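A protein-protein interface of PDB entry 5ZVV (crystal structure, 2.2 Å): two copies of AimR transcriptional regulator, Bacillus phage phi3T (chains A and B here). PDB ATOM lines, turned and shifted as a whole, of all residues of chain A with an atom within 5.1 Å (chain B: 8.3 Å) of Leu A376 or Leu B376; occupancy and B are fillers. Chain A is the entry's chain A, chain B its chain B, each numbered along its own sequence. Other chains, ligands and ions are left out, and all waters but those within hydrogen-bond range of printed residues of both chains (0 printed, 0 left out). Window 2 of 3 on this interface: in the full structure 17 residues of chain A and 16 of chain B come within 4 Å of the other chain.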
ATOM      1  N   TYR A 345      15.473  -0.698 -15.569  1.00  0.00           N
ATOM      2  CA  TYR A 345      15.660   0.740 -15.393  1.00  0.00           C
ATOM      3  C   TYR A 345      15.059   1.207 -14.073  1.00  0.00           C
ATOM      4  O   TYR A 345      15.689   1.962 -13.320  1.00  0.00           O
ATOM      5  CB  TYR A 345      15.038   1.501 -16.565  1.00  0.00           C
ATOM      6  CG  TYR A 345      15.611   1.152 -17.924  1.00  0.00           C
ATOM      7  CD1 TYR A 345      16.895   0.632 -18.049  1.00  0.00           C
ATOM      8  CD2 TYR A 345      14.868   1.346 -19.082  1.00  0.00           C
ATOM      9  CE1 TYR A 345      17.421   0.314 -19.288  1.00  0.00           C
ATOM     10  CE2 TYR A 345      15.384   1.029 -20.324  1.00  0.00           C
ATOM     11  CZ  TYR A 345      16.661   0.515 -20.421  1.00  0.00           C
ATOM     12  OH  TYR A 345      17.179   0.199 -21.655  1.00  0.00           O
ATOM     13  N   LEU A 367      21.543  -6.064 -17.609  1.00  0.00           N
ATOM     14  CA  LEU A 367      21.640  -5.229 -18.801  1.00  0.00           C
ATOM     15  C   LEU A 367      22.892  -5.558 -19.600  1.00  0.00           C
ATOM     16  O   LEU A 367      22.890  -5.445 -20.831  1.00  0.00           O
ATOM     17  CB  LEU A 367      21.623  -3.749 -18.415  1.00  0.00           C
ATOM     18  CG  LEU A 367      20.293  -3.186 -17.907  1.00  0.00           C
ATOM     19  CD1 LEU A 367      20.443  -1.725 -17.513  1.00  0.00           C
ATOM     20  CD2 LEU A 367      19.204  -3.344 -18.956  1.00  0.00           C
ATOM     21  N   ALA A 372      24.144  -4.381 -23.461  1.00  0.00           N
ATOM     22  CA  ALA A 372      24.260  -2.951 -23.226  1.00  0.00           C
ATOM     23  C   ALA A 372      25.727  -2.531 -23.237  1.00  0.00           C
ATOM     24  O   ALA A 372      26.631  -3.330 -22.976  1.00  0.00           O
ATOM     25  CB  ALA A 372      23.614  -2.562 -21.895  1.00  0.00           C
ATOM     26  N   ASP A 373      25.953  -1.258 -23.552  1.00  0.00           N
ATOM     27  CA  ASP A 373      27.303  -0.711 -23.555  1.00  0.00           C
ATOM     28  C   ASP A 373      27.889  -0.765 -22.150  1.00  0.00           C
ATOM     29  O   ASP A 373      27.390  -0.105 -21.233  1.00  0.00           O
ATOM     30  CB  ASP A 373      27.285   0.725 -24.080  1.00  0.00           C
ATOM     31  CG  ASP A 373      28.673   1.262 -24.378  1.00  0.00           C
ATOM     32  OD1 ASP A 373      29.672   0.612 -24.006  1.00  0.00           O
ATOM     33  OD2 ASP A 373      28.765   2.342 -24.996  1.00  0.00           O
ATOM     34  N   LEU A 374      28.954  -1.553 -21.988  1.00  0.00           N
ATOM     35  CA  LEU A 374      29.530  -1.771 -20.665  1.00  0.00           C
ATOM     36  C   LEU A 374      30.074  -0.482 -20.063  1.00  0.00           C
ATOM     37  O   LEU A 374      30.090  -0.332 -18.835  1.00  0.00           O
ATOM     38  CB  LEU A 374      30.630  -2.830 -20.747  1.00  0.00           C
ATOM     39  CG  LEU A 374      31.270  -3.269 -19.431  1.00  0.00           C
ATOM     40  CD1 LEU A 374      30.209  -3.778 -18.469  1.00  0.00           C
ATOM     41  CD2 LEU A 374      32.326  -4.335 -19.682  1.00  0.00           C
ATOM     42  N   GLU A 375      30.523   0.456 -20.898  1.00  0.00           N
ATOM     43  CA  GLU A 375      31.026   1.723 -20.376  1.00  0.00           C
ATOM     44  C   GLU A 375      29.893   2.582 -19.828  1.00  0.00           C
ATOM     45  O   GLU A 375      30.023   3.185 -18.754  1.00  0.00           O
ATOM     46  CB  GLU A 375      31.802   2.466 -21.464  1.00  0.00           C
ATOM     47  CG  GLU A 375      33.188   1.896 -21.718  1.00  0.00           C
ATOM     48  CD  GLU A 375      33.841   2.476 -22.956  1.00  0.00           C
ATOM     49  OE1 GLU A 375      33.187   2.493 -24.021  1.00  0.00           O
ATOM     50  OE2 GLU A 375      35.004   2.921 -22.861  1.00  0.00           O
ATOM     51  N   LEU A 376      28.769   2.645 -20.548  1.00  0.00           N
ATOM     52  CA  LEU A 376      27.599   3.344 -20.028  1.00  0.00           C
ATOM     53  C   LEU A 376      27.109   2.702 -18.737  1.00  0.00           C
ATOM     54  O   LEU A 376      26.733   3.403 -17.791  1.00  0.00           O
ATOM     55  CB  LEU A 376      26.486   3.366 -21.075  1.00  0.00           C
ATOM     56  CG  LEU A 376      26.802   4.103 -22.378  1.00  0.00           C
ATOM     57  CD1 LEU A 376      25.553   4.255 -23.229  1.00  0.00           C
ATOM     58  CD2 LEU A 376      27.428   5.458 -22.088  1.00  0.00           C
ATOM     59  N   LEU A 377      27.117   1.368 -18.677  1.00  0.00           N
ATOM     60  CA  LEU A 377      26.721   0.680 -17.452  1.00  0.00           C
ATOM     61  C   LEU A 377      27.663   1.015 -16.303  1.00  0.00           C
ATOM     62  O   LEU A 377      27.220   1.213 -15.166  1.00  0.00           O
ATOM     63  CB  LEU A 377      26.680  -0.829 -17.689  1.00  0.00           C
ATOM     64  CG  LEU A 377      25.683  -1.323 -18.737  1.00  0.00           C
ATOM     65  CD1 LEU A 377      25.789  -2.827 -18.895  1.00  0.00           C
ATOM     66  CD2 LEU A 377      24.264  -0.918 -18.369  1.00  0.00           C
ATOM     67  N   ASN A 378      28.968   1.086 -16.581  1.00  0.00           N
ATOM     68  CA  ASN A 378      29.925   1.460 -15.546  1.00  0.00           C
ATOM     69  C   ASN A 378      29.711   2.892 -15.077  1.00  0.00           C
ATOM     70  O   ASN A 378      29.945   3.200 -13.903  1.00  0.00           O
ATOM     71  CB  ASN A 378      31.354   1.276 -16.056  1.00  0.00           C
ATOM     72  CG  ASN A 378      31.757  -0.183 -16.141  1.00  0.00           C
ATOM     73  OD1 ASN A 378      31.303  -1.011 -15.351  1.00  0.00           O
ATOM     74  ND2 ASN A 378      32.617  -0.505 -17.101  1.00  0.00           N
ATOM     75  N   LEU A 379      29.272   3.779 -15.973  1.00  0.00           N
ATOM     76  CA  LEU A 379      28.942   5.135 -15.548  1.00  0.00           C
ATOM     77  C   LEU A 379      27.674   5.164 -14.703  1.00  0.00           C
ATOM     78  O   LEU A 379      27.559   5.986 -13.788  1.00  0.00           O
ATOM     79  CB  LEU A 379      28.795   6.048 -16.764  1.00  0.00           C
ATOM     80  CG  LEU A 379      30.056   6.275 -17.601  1.00  0.00           C
ATOM     81  CD1 LEU A 379      29.730   7.091 -18.843  1.00  0.00           C
ATOM     82  CD2 LEU A 379      31.141   6.955 -16.777  1.00  0.00           C
ATOM     83  N   ILE A 380      26.717   4.277 -14.990  1.00  0.00           N
ATOM     84  CA  ILE A 380      25.490   4.227 -14.202  1.00  0.00           C
ATOM     85  C   ILE A 380      25.769   3.731 -12.788  1.00  0.00           C
ATOM     86  O   ILE A 380      25.148   4.198 -11.827  1.00  0.00           O
ATOM     87  CB  ILE A 380      24.438   3.349 -14.909  1.00  0.00           C
ATOM     88  CG1 ILE A 380      24.059   3.949 -16.262  1.00  0.00           C
ATOM     89  CG2 ILE A 380      23.192   3.190 -14.046  1.00  0.00           C
ATOM     90  CD1 ILE A 380      23.209   3.035 -17.113  1.00  0.00           C
ATOM     91  N   LYS B 341      34.939   9.923 -27.075  1.00  0.00           N
ATOM     92  CA  LYS B 341      33.993   9.571 -26.021  1.00  0.00           C
ATOM     93  C   LYS B 341      34.652   9.543 -24.647  1.00  0.00           C
ATOM     94  O   LYS B 341      33.973   9.747 -23.634  1.00  0.00           O
ATOM     95  CB  LYS B 341      33.353   8.215 -26.323  1.00  0.00           C
ATOM     96  CG  LYS B 341      32.329   8.238 -27.443  1.00  0.00           C
ATOM     97  CD  LYS B 341      31.695   6.867 -27.618  1.00  0.00           C
ATOM     98  CE  LYS B 341      30.551   6.900 -28.616  1.00  0.00           C
ATOM     99  NZ  LYS B 341      29.958   5.548 -28.804  1.00  0.00           N
ATOM    100  N   TYR B 345      33.362  10.780 -20.992  1.00  0.00           N
ATOM    101  CA  TYR B 345      33.302   9.910 -19.820  1.00  0.00           C
ATOM    102  C   TYR B 345      33.982  10.557 -18.621  1.00  0.00           C
ATOM    103  O   TYR B 345      33.458  10.511 -17.501  1.00  0.00           O
ATOM    104  CB  TYR B 345      33.948   8.559 -20.130  1.00  0.00           C
ATOM    105  CG  TYR B 345      33.250   7.762 -21.211  1.00  0.00           C
ATOM    106  CD1 TYR B 345      31.913   7.989 -21.520  1.00  0.00           C
ATOM    107  CD2 TYR B 345      33.927   6.779 -21.920  1.00  0.00           C
ATOM    108  CE1 TYR B 345      31.276   7.262 -22.508  1.00  0.00           C
ATOM    109  CE2 TYR B 345      33.296   6.047 -22.907  1.00  0.00           C
ATOM    110  CZ  TYR B 345      31.972   6.293 -23.197  1.00  0.00           C
ATOM    111  OH  TYR B 345      31.345   5.564 -24.178  1.00  0.00           O
ATOM    112  N   ILE B 348      31.754  13.240 -17.336  1.00  0.00           N
ATOM    113  CA  ILE B 348      30.671  12.643 -16.559  1.00  0.00           C
ATOM    114  C   ILE B 348      31.154  12.290 -15.157  1.00  0.00           C
ATOM    115  O   ILE B 348      30.495  12.600 -14.157  1.00  0.00           O
ATOM    116  CB  ILE B 348      30.107  11.412 -17.289  1.00  0.00           C
ATOM    117  CG1 ILE B 348      29.240  11.846 -18.472  1.00  0.00           C
ATOM    118  CG2 ILE B 348      29.322  10.524 -16.328  1.00  0.00           C
ATOM    119  CD1 ILE B 348      28.859  10.717 -19.391  1.00  0.00           C
ATOM    120  N   ARG B 349      32.321  11.644 -15.064  1.00  0.00           N
ATOM    121  CA  ARG B 349      32.827  11.225 -13.760  1.00  0.00           C
ATOM    122  C   ARG B 349      33.106  12.421 -12.860  1.00  0.00           C
ATOM    123  O   ARG B 349      32.869  12.362 -11.648  1.00  0.00           O
ATOM    124  CB  ARG B 349      34.087  10.375 -13.925  1.00  0.00           C
ATOM    125  CG  ARG B 349      33.862   9.059 -14.653  1.00  0.00           C
ATOM    126  CD  ARG B 349      35.113   8.197 -14.631  1.00  0.00           C
ATOM    127  NE  ARG B 349      34.992   7.035 -15.507  1.00  0.00           N
ATOM    128  CZ  ARG B 349      35.424   7.000 -16.764  1.00  0.00           C
ATOM    129  NH1 ARG B 349      36.014   8.065 -17.293  1.00  0.00           N
ATOM    130  NH2 ARG B 349      35.273   5.902 -17.492  1.00  0.00           N
ATOM    131  N   LYS B 352      29.867  13.815 -11.599  1.00  0.00           N
ATOM    132  CA  LYS B 352      29.333  12.970 -10.537  1.00  0.00           C
ATOM    133  C   LYS B 352      30.102  13.163  -9.235  1.00  0.00           C
ATOM    134  O   LYS B 352      29.502  13.199  -8.155  1.00  0.00           O
ATOM    135  CB  LYS B 352      29.359  11.505 -10.966  1.00  0.00           C
ATOM    136  CG  LYS B 352      28.213  11.104 -11.873  1.00  0.00           C
ATOM    137  CD  LYS B 352      28.363   9.665 -12.332  1.00  0.00           C
ATOM    138  CE  LYS B 352      27.091   9.152 -12.987  1.00  0.00           C
ATOM    139  NZ  LYS B 352      25.968   9.060 -12.013  1.00  0.00           N
ATOM    140  N   LEU B 364      26.449  14.052 -21.838  1.00  0.00           N
ATOM    141  CA  LEU B 364      25.385  13.116 -22.194  1.00  0.00           C
ATOM    142  C   LEU B 364      24.732  13.504 -23.518  1.00  0.00           C
ATOM    143  O   LEU B 364      24.597  12.671 -24.424  1.00  0.00           O
ATOM    144  CB  LEU B 364      24.344  13.051 -21.074  1.00  0.00           C
ATOM    145  CG  LEU B 364      24.804  12.469 -19.736  1.00  0.00           C
ATOM    146  CD1 LEU B 364      23.699  12.576 -18.699  1.00  0.00           C
ATOM    147  CD2 LEU B 364      25.251  11.023 -19.894  1.00  0.00           C
ATOM    148  N   LEU B 367      26.979  12.525 -26.144  1.00  0.00           N
ATOM    149  CA  LEU B 367      26.988  11.082 -26.356  1.00  0.00           C
ATOM    150  C   LEU B 367      25.738  10.624 -27.092  1.00  0.00           C
ATOM    151  O   LEU B 367      25.801   9.686 -27.895  1.00  0.00           O
ATOM    152  CB  LEU B 367      27.124  10.350 -25.021  1.00  0.00           C
ATOM    153  CG  LEU B 367      28.469  10.486 -24.304  1.00  0.00           C
ATOM    154  CD1 LEU B 367      28.441   9.769 -22.964  1.00  0.00           C
ATOM    155  CD2 LEU B 367      29.597   9.951 -25.175  1.00  0.00           C
ATOM    156  N   GLU B 368      24.605  11.285 -26.848  1.00  0.00           N
ATOM    157  CA  GLU B 368      23.354  10.899 -27.492  1.00  0.00           C
ATOM    158  C   GLU B 368      23.422  11.097 -29.001  1.00  0.00           C
ATOM    159  O   GLU B 368      23.032  10.210 -29.770  1.00  0.00           O
ATOM    160  CB  GLU B 368      22.197  11.698 -26.896  1.00  0.00           C
ATOM    161  CG  GLU B 368      20.838  11.337 -27.458  1.00  0.00           C
ATOM    162  CD  GLU B 368      19.733  12.185 -26.873  1.00  0.00           C
ATOM    163  OE1 GLU B 368      18.616  12.176 -27.430  1.00  0.00           O
ATOM    164  OE2 GLU B 368      19.985  12.865 -25.856  1.00  0.00           O
ATOM    165  N   GLY B 371      25.108   8.535 -31.072  1.00  0.00           N
ATOM    166  CA  GLY B 371      24.437   7.254 -31.171  1.00  0.00           C
ATOM    167  C   GLY B 371      24.420   6.414 -29.914  1.00  0.00           C
ATOM    168  O   GLY B 371      24.251   5.193 -30.008  1.00  0.00           O
ATOM    169  N   ALA B 372      24.584   7.018 -28.740  1.00  0.00           N
ATOM    170  CA  ALA B 372      24.545   6.261 -27.498  1.00  0.00           C
ATOM    171  C   ALA B 372      23.103   6.000 -27.081  1.00  0.00           C
ATOM    172  O   ALA B 372      22.191   6.766 -27.406  1.00  0.00           O
ATOM    173  CB  ALA B 372      25.287   7.003 -26.386  1.00  0.00           C
ATOM    174  N   ASP B 373      22.902   4.899 -26.360  1.00  0.00           N
ATOM    175  CA  ASP B 373      21.566   4.525 -25.916  1.00  0.00           C
ATOM    176  C   ASP B 373      21.008   5.590 -24.979  1.00  0.00           C
ATOM    177  O   ASP B 373      21.620   5.910 -23.957  1.00  0.00           O
ATOM    178  CB  ASP B 373      21.612   3.164 -25.223  1.00  0.00           C
ATOM    179  CG  ASP B 373      20.237   2.566 -25.021  1.00  0.00           C
ATOM    180  OD1 ASP B 373      19.240   3.225 -25.382  1.00  0.00           O
ATOM    181  OD2 ASP B 373      20.154   1.431 -24.505  1.00  0.00           O
ATOM    182  N   LEU B 374      19.834   6.131 -25.327  1.00  0.00           N
ATOM    183  CA  LEU B 374      19.306   7.286 -24.603  1.00  0.00           C
ATOM    184  C   LEU B 374      18.915   6.931 -23.174  1.00  0.00           C
ATOM    185  O   LEU B 374      19.208   7.688 -22.243  1.00  0.00           O
ATOM    186  CB  LEU B 374      18.107   7.885 -25.343  1.00  0.00           C
ATOM    187  CG  LEU B 374      17.401   9.040 -24.617  1.00  0.00           C
ATOM    188  CD1 LEU B 374      18.363  10.193 -24.349  1.00  0.00           C
ATOM    189  CD2 LEU B 374      16.175   9.531 -25.381  1.00  0.00           C
ATOM    190  N   GLU B 375      18.243   5.795 -22.974  1.00  0.00           N
ATOM    191  CA  GLU B 375      17.769   5.457 -21.632  1.00  0.00           C
ATOM    192  C   GLU B 375      18.930   5.234 -20.672  1.00  0.00           C
ATOM    193  O   GLU B 375      18.856   5.611 -19.495  1.00  0.00           O
ATOM    194  CB  GLU B 375      16.856   4.232 -21.683  1.00  0.00           C
ATOM    195  CG  GLU B 375      17.236   3.195 -22.728  1.00  0.00           C
ATOM    196  CD  GLU B 375      16.258   3.151 -23.888  1.00  0.00           C
ATOM    197  OE1 GLU B 375      16.186   4.139 -24.651  1.00  0.00           O
ATOM    198  OE2 GLU B 375      15.554   2.128 -24.030  1.00  0.00           O
ATOM    199  N   LEU B 376      20.014   4.631 -21.159  1.00  0.00           N
ATOM    200  CA  LEU B 376      21.216   4.498 -20.343  1.00  0.00           C
ATOM    201  C   LEU B 376      21.766   5.866 -19.958  1.00  0.00           C
ATOM    202  O   LEU B 376      22.180   6.084 -18.812  1.00  0.00           O
ATOM    203  CB  LEU B 376      22.276   3.682 -21.094  1.00  0.00           C
ATOM    204  CG  LEU B 376      22.271   2.150 -20.985  1.00  0.00           C
ATOM    205  CD1 LEU B 376      20.889   1.543 -21.182  1.00  0.00           C
ATOM    206  CD2 LEU B 376      23.251   1.537 -21.978  1.00  0.00           C
ATOM    207  N   LEU B 377      21.762   6.809 -20.905  1.00  0.00           N
ATOM    208  CA  LEU B 377      22.233   8.160 -20.614  1.00  0.00           C
ATOM    209  C   LEU B 377      21.357   8.831 -19.568  1.00  0.00           C
ATOM    210  O   LEU B 377      21.853   9.555 -18.697  1.00  0.00           O
ATOM    211  CB  LEU B 377      22.270   8.990 -21.899  1.00  0.00           C
ATOM    212  CG  LEU B 377      23.208   8.482 -22.993  1.00  0.00           C
ATOM    213  CD1 LEU B 377      22.988   9.238 -24.290  1.00  0.00           C
ATOM    214  CD2 LEU B 377      24.664   8.577 -22.562  1.00  0.00           C
ATOM    215  N   ASN B 378      20.045   8.603 -19.641  1.00  0.00           N
ATOM    216  CA  ASN B 378      19.151   9.113 -18.610  1.00  0.00           C
ATOM    217  C   ASN B 378      19.477   8.500 -17.257  1.00  0.00           C
ATOM    218  O   ASN B 378      19.372   9.170 -16.221  1.00  0.00           O
ATOM    219  CB  ASN B 378      17.695   8.839 -18.986  1.00  0.00           C
ATOM    220  CG  ASN B 378      17.262   9.585 -20.234  1.00  0.00           C
ATOM    221  OD1 ASN B 378      17.760  10.673 -20.531  1.00  0.00           O
ATOM    222  ND2 ASN B 378      16.320   9.005 -20.967  1.00  0.00           N
ATOM    223  N   LEU B 379      19.877   7.227 -17.246  1.00  0.00           N
ATOM    224  CA  LEU B 379      20.266   6.600 -15.986  1.00  0.00           C
ATOM    225  C   LEU B 379      21.587   7.155 -15.465  1.00  0.00           C
ATOM    226  O   LEU B 379      21.832   7.133 -14.252  1.00  0.00           O
ATOM    227  CB  LEU B 379      20.358   5.083 -16.153  1.00  0.00           C
ATOM    228  CG  LEU B 379      19.064   4.367 -16.547  1.00  0.00           C
ATOM    229  CD1 LEU B 379      19.315   2.880 -16.733  1.00  0.00           C
ATOM    230  CD2 LEU B 379      17.968   4.607 -15.518  1.00  0.00           C
ATOM    231  N   ILE B 380      22.450   7.650 -16.358  1.00  0.00           N
ATOM    232  CA  ILE B 380      23.691   8.268 -15.903  1.00  0.00           C
ATOM    233  C   ILE B 380      23.408   9.596 -15.208  1.00  0.00           C
ATOM    234  O   ILE B 380      24.119   9.978 -14.268  1.00  0.00           O
ATOM    235  CB  ILE B 380      24.667   8.446 -17.084  1.00  0.00           C
ATOM    236  CG1 ILE B 380      25.029   7.089 -17.691  1.00  0.00           C
ATOM    237  CG2 ILE B 380      25.928   9.169 -16.640  1.00  0.00           C
ATOM    238  CD1 ILE B 380      25.870   7.183 -18.944  1.00  0.00           C
ATOM    239  N   SER B 381      22.366  10.308 -15.633  1.00  0.00           N
ATOM    240  CA  SER B 381      22.108  11.657 -15.141  1.00  0.00           C
ATOM    241  C   SER B 381      21.511  11.692 -13.740  1.00  0.00           C
ATOM    242  O   SER B 381      21.298  12.787 -13.210  1.00  0.00           O
ATOM    243  CB  SER B 381      21.176  12.402 -16.101  1.00  0.00           C
ATOM    244  OG  SER B 381      19.873  11.850 -16.075  1.00  0.00           O
ATOM    245  N   ILE B 382      21.234  10.545 -13.130  1.00  0.00           N
ATOM    246  CA  ILE B 382      20.629  10.527 -11.802  1.00  0.00           C
ATOM    247  C   ILE B 382      21.534   9.820 -10.800  1.00  0.00           C
ATOM    248  O   ILE B 382      22.758   9.932 -10.866  1.00  0.00           O
ATOM    249  CB  ILE B 382      19.230   9.877 -11.844  1.00  0.00           C
ATOM    250  CG1 ILE B 382      19.274   8.539 -12.587  1.00  0.00           C
ATOM    251  CG2 ILE B 382      18.227  10.812 -12.503  1.00  0.00           C
ATOM    252  CD1 ILE B 382      19.423   7.332 -11.688  1.00  0.00           C
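Among the printed residues, pairs that only touch across the chains: Leu A379 with Lys B352 (3.3 Å), Tyr A345 with Leu B379 (3.6 Å), Glu A375 with Tyr B345 (3.6 Å), Leu A379 with Tyr B345 (3.6 Å), Ile A380 with Ile B380 (3.6 Å), Ile A380 with Leu B376 (3.6 Å), Ile A380 with Leu B379 (3.6 Å), Leu A379 with Ile B348 (3.8 Å), Leu A376 with Leu B376 (3.8 Å), Leu A379 with Ile B380 (3.8 Å), Leu A376 with Ile B380 (3.9 Å) and Tyr A345 with Leu B376 (3.97 Å).
Leu A376 touches just these residues of chain B: Leu B376 (3.8 Å) and Ile B380 (3.9 Å).
Printed residues of chain A within 4 Å of Leu B379: Tyr A345 (3.6 Å) and Ile A380 (3.6 Å).
Printed residues of chain A within 4 Å of Tyr B345: Glu A375 and Leu A379.
Of the printed residues of chain A, Glu B375 touches Tyr A345.
Of the printed residues of chain B, Tyr A345 touches Glu B375 (3.2 Å), Leu B376 (3.97 Å) and Leu B379 (3.6 Å).
Of the printed residues of chain B, Ile A380 touches Leu B376 (3.6 Å), Leu B379 (3.6 Å) and Ile B380 (3.6 Å).
Leu B377 touches none of the printed residues of chain A.
Asn A378 touches none of the printed residues of chain B.
The nearest residue of chain B that does not touch Leu A376 is Asp B373 (4.2 Å).
The nearest residue of chain A that does not touch Leu B376 is Ala A372 (4.1 Å).
The nearest printed residue of chain B that does not touch Leu A379 is Arg B349 (4.04 Å).
Tyr A345 touches Glu B375, and with the chains exchanged Glu A375 touches Tyr B345.
Tyr A345 touches Leu B379, and with the chains exchanged Leu A379 touches Tyr B345.
Leu B376 touches its own counterpart, Leu A376.
Ile B380 touches its own counterpart, Ile A380.
OH of Tyr A345 lies close to OE2 of Glu B375 (3.5 Å).
The side-chain carboxylate of Asp A373 sits close to the backbone NH of Glu A375 (3.2 Å).
The side-chain amino group of Lys B352 sits at hydrogen-bond distance from the backbone carbonyl oxygen of Ile B380, at 3.1 Å.
Of the 11 printed residues of chain A, 5 touch a printed residue of chain B.
Printed residues of chain A that touch a printed residue of chain B: Tyr A345, Glu A375, Leu A376, Leu A379 and Ile A380.
Hydrophobic or aromatic side chains of chain A within 4 Å of the printed part of chain B: Tyr A345, Leu A376, Leu A379 and Ile A380.
Of the 20 printed residues of chain B, 7 touch a printed residue of chain A.
Among the printed residues, no Asp or Glu carboxylate lies within 4 Å of a Lys or Arg side-chain nitrogen of the other chain.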
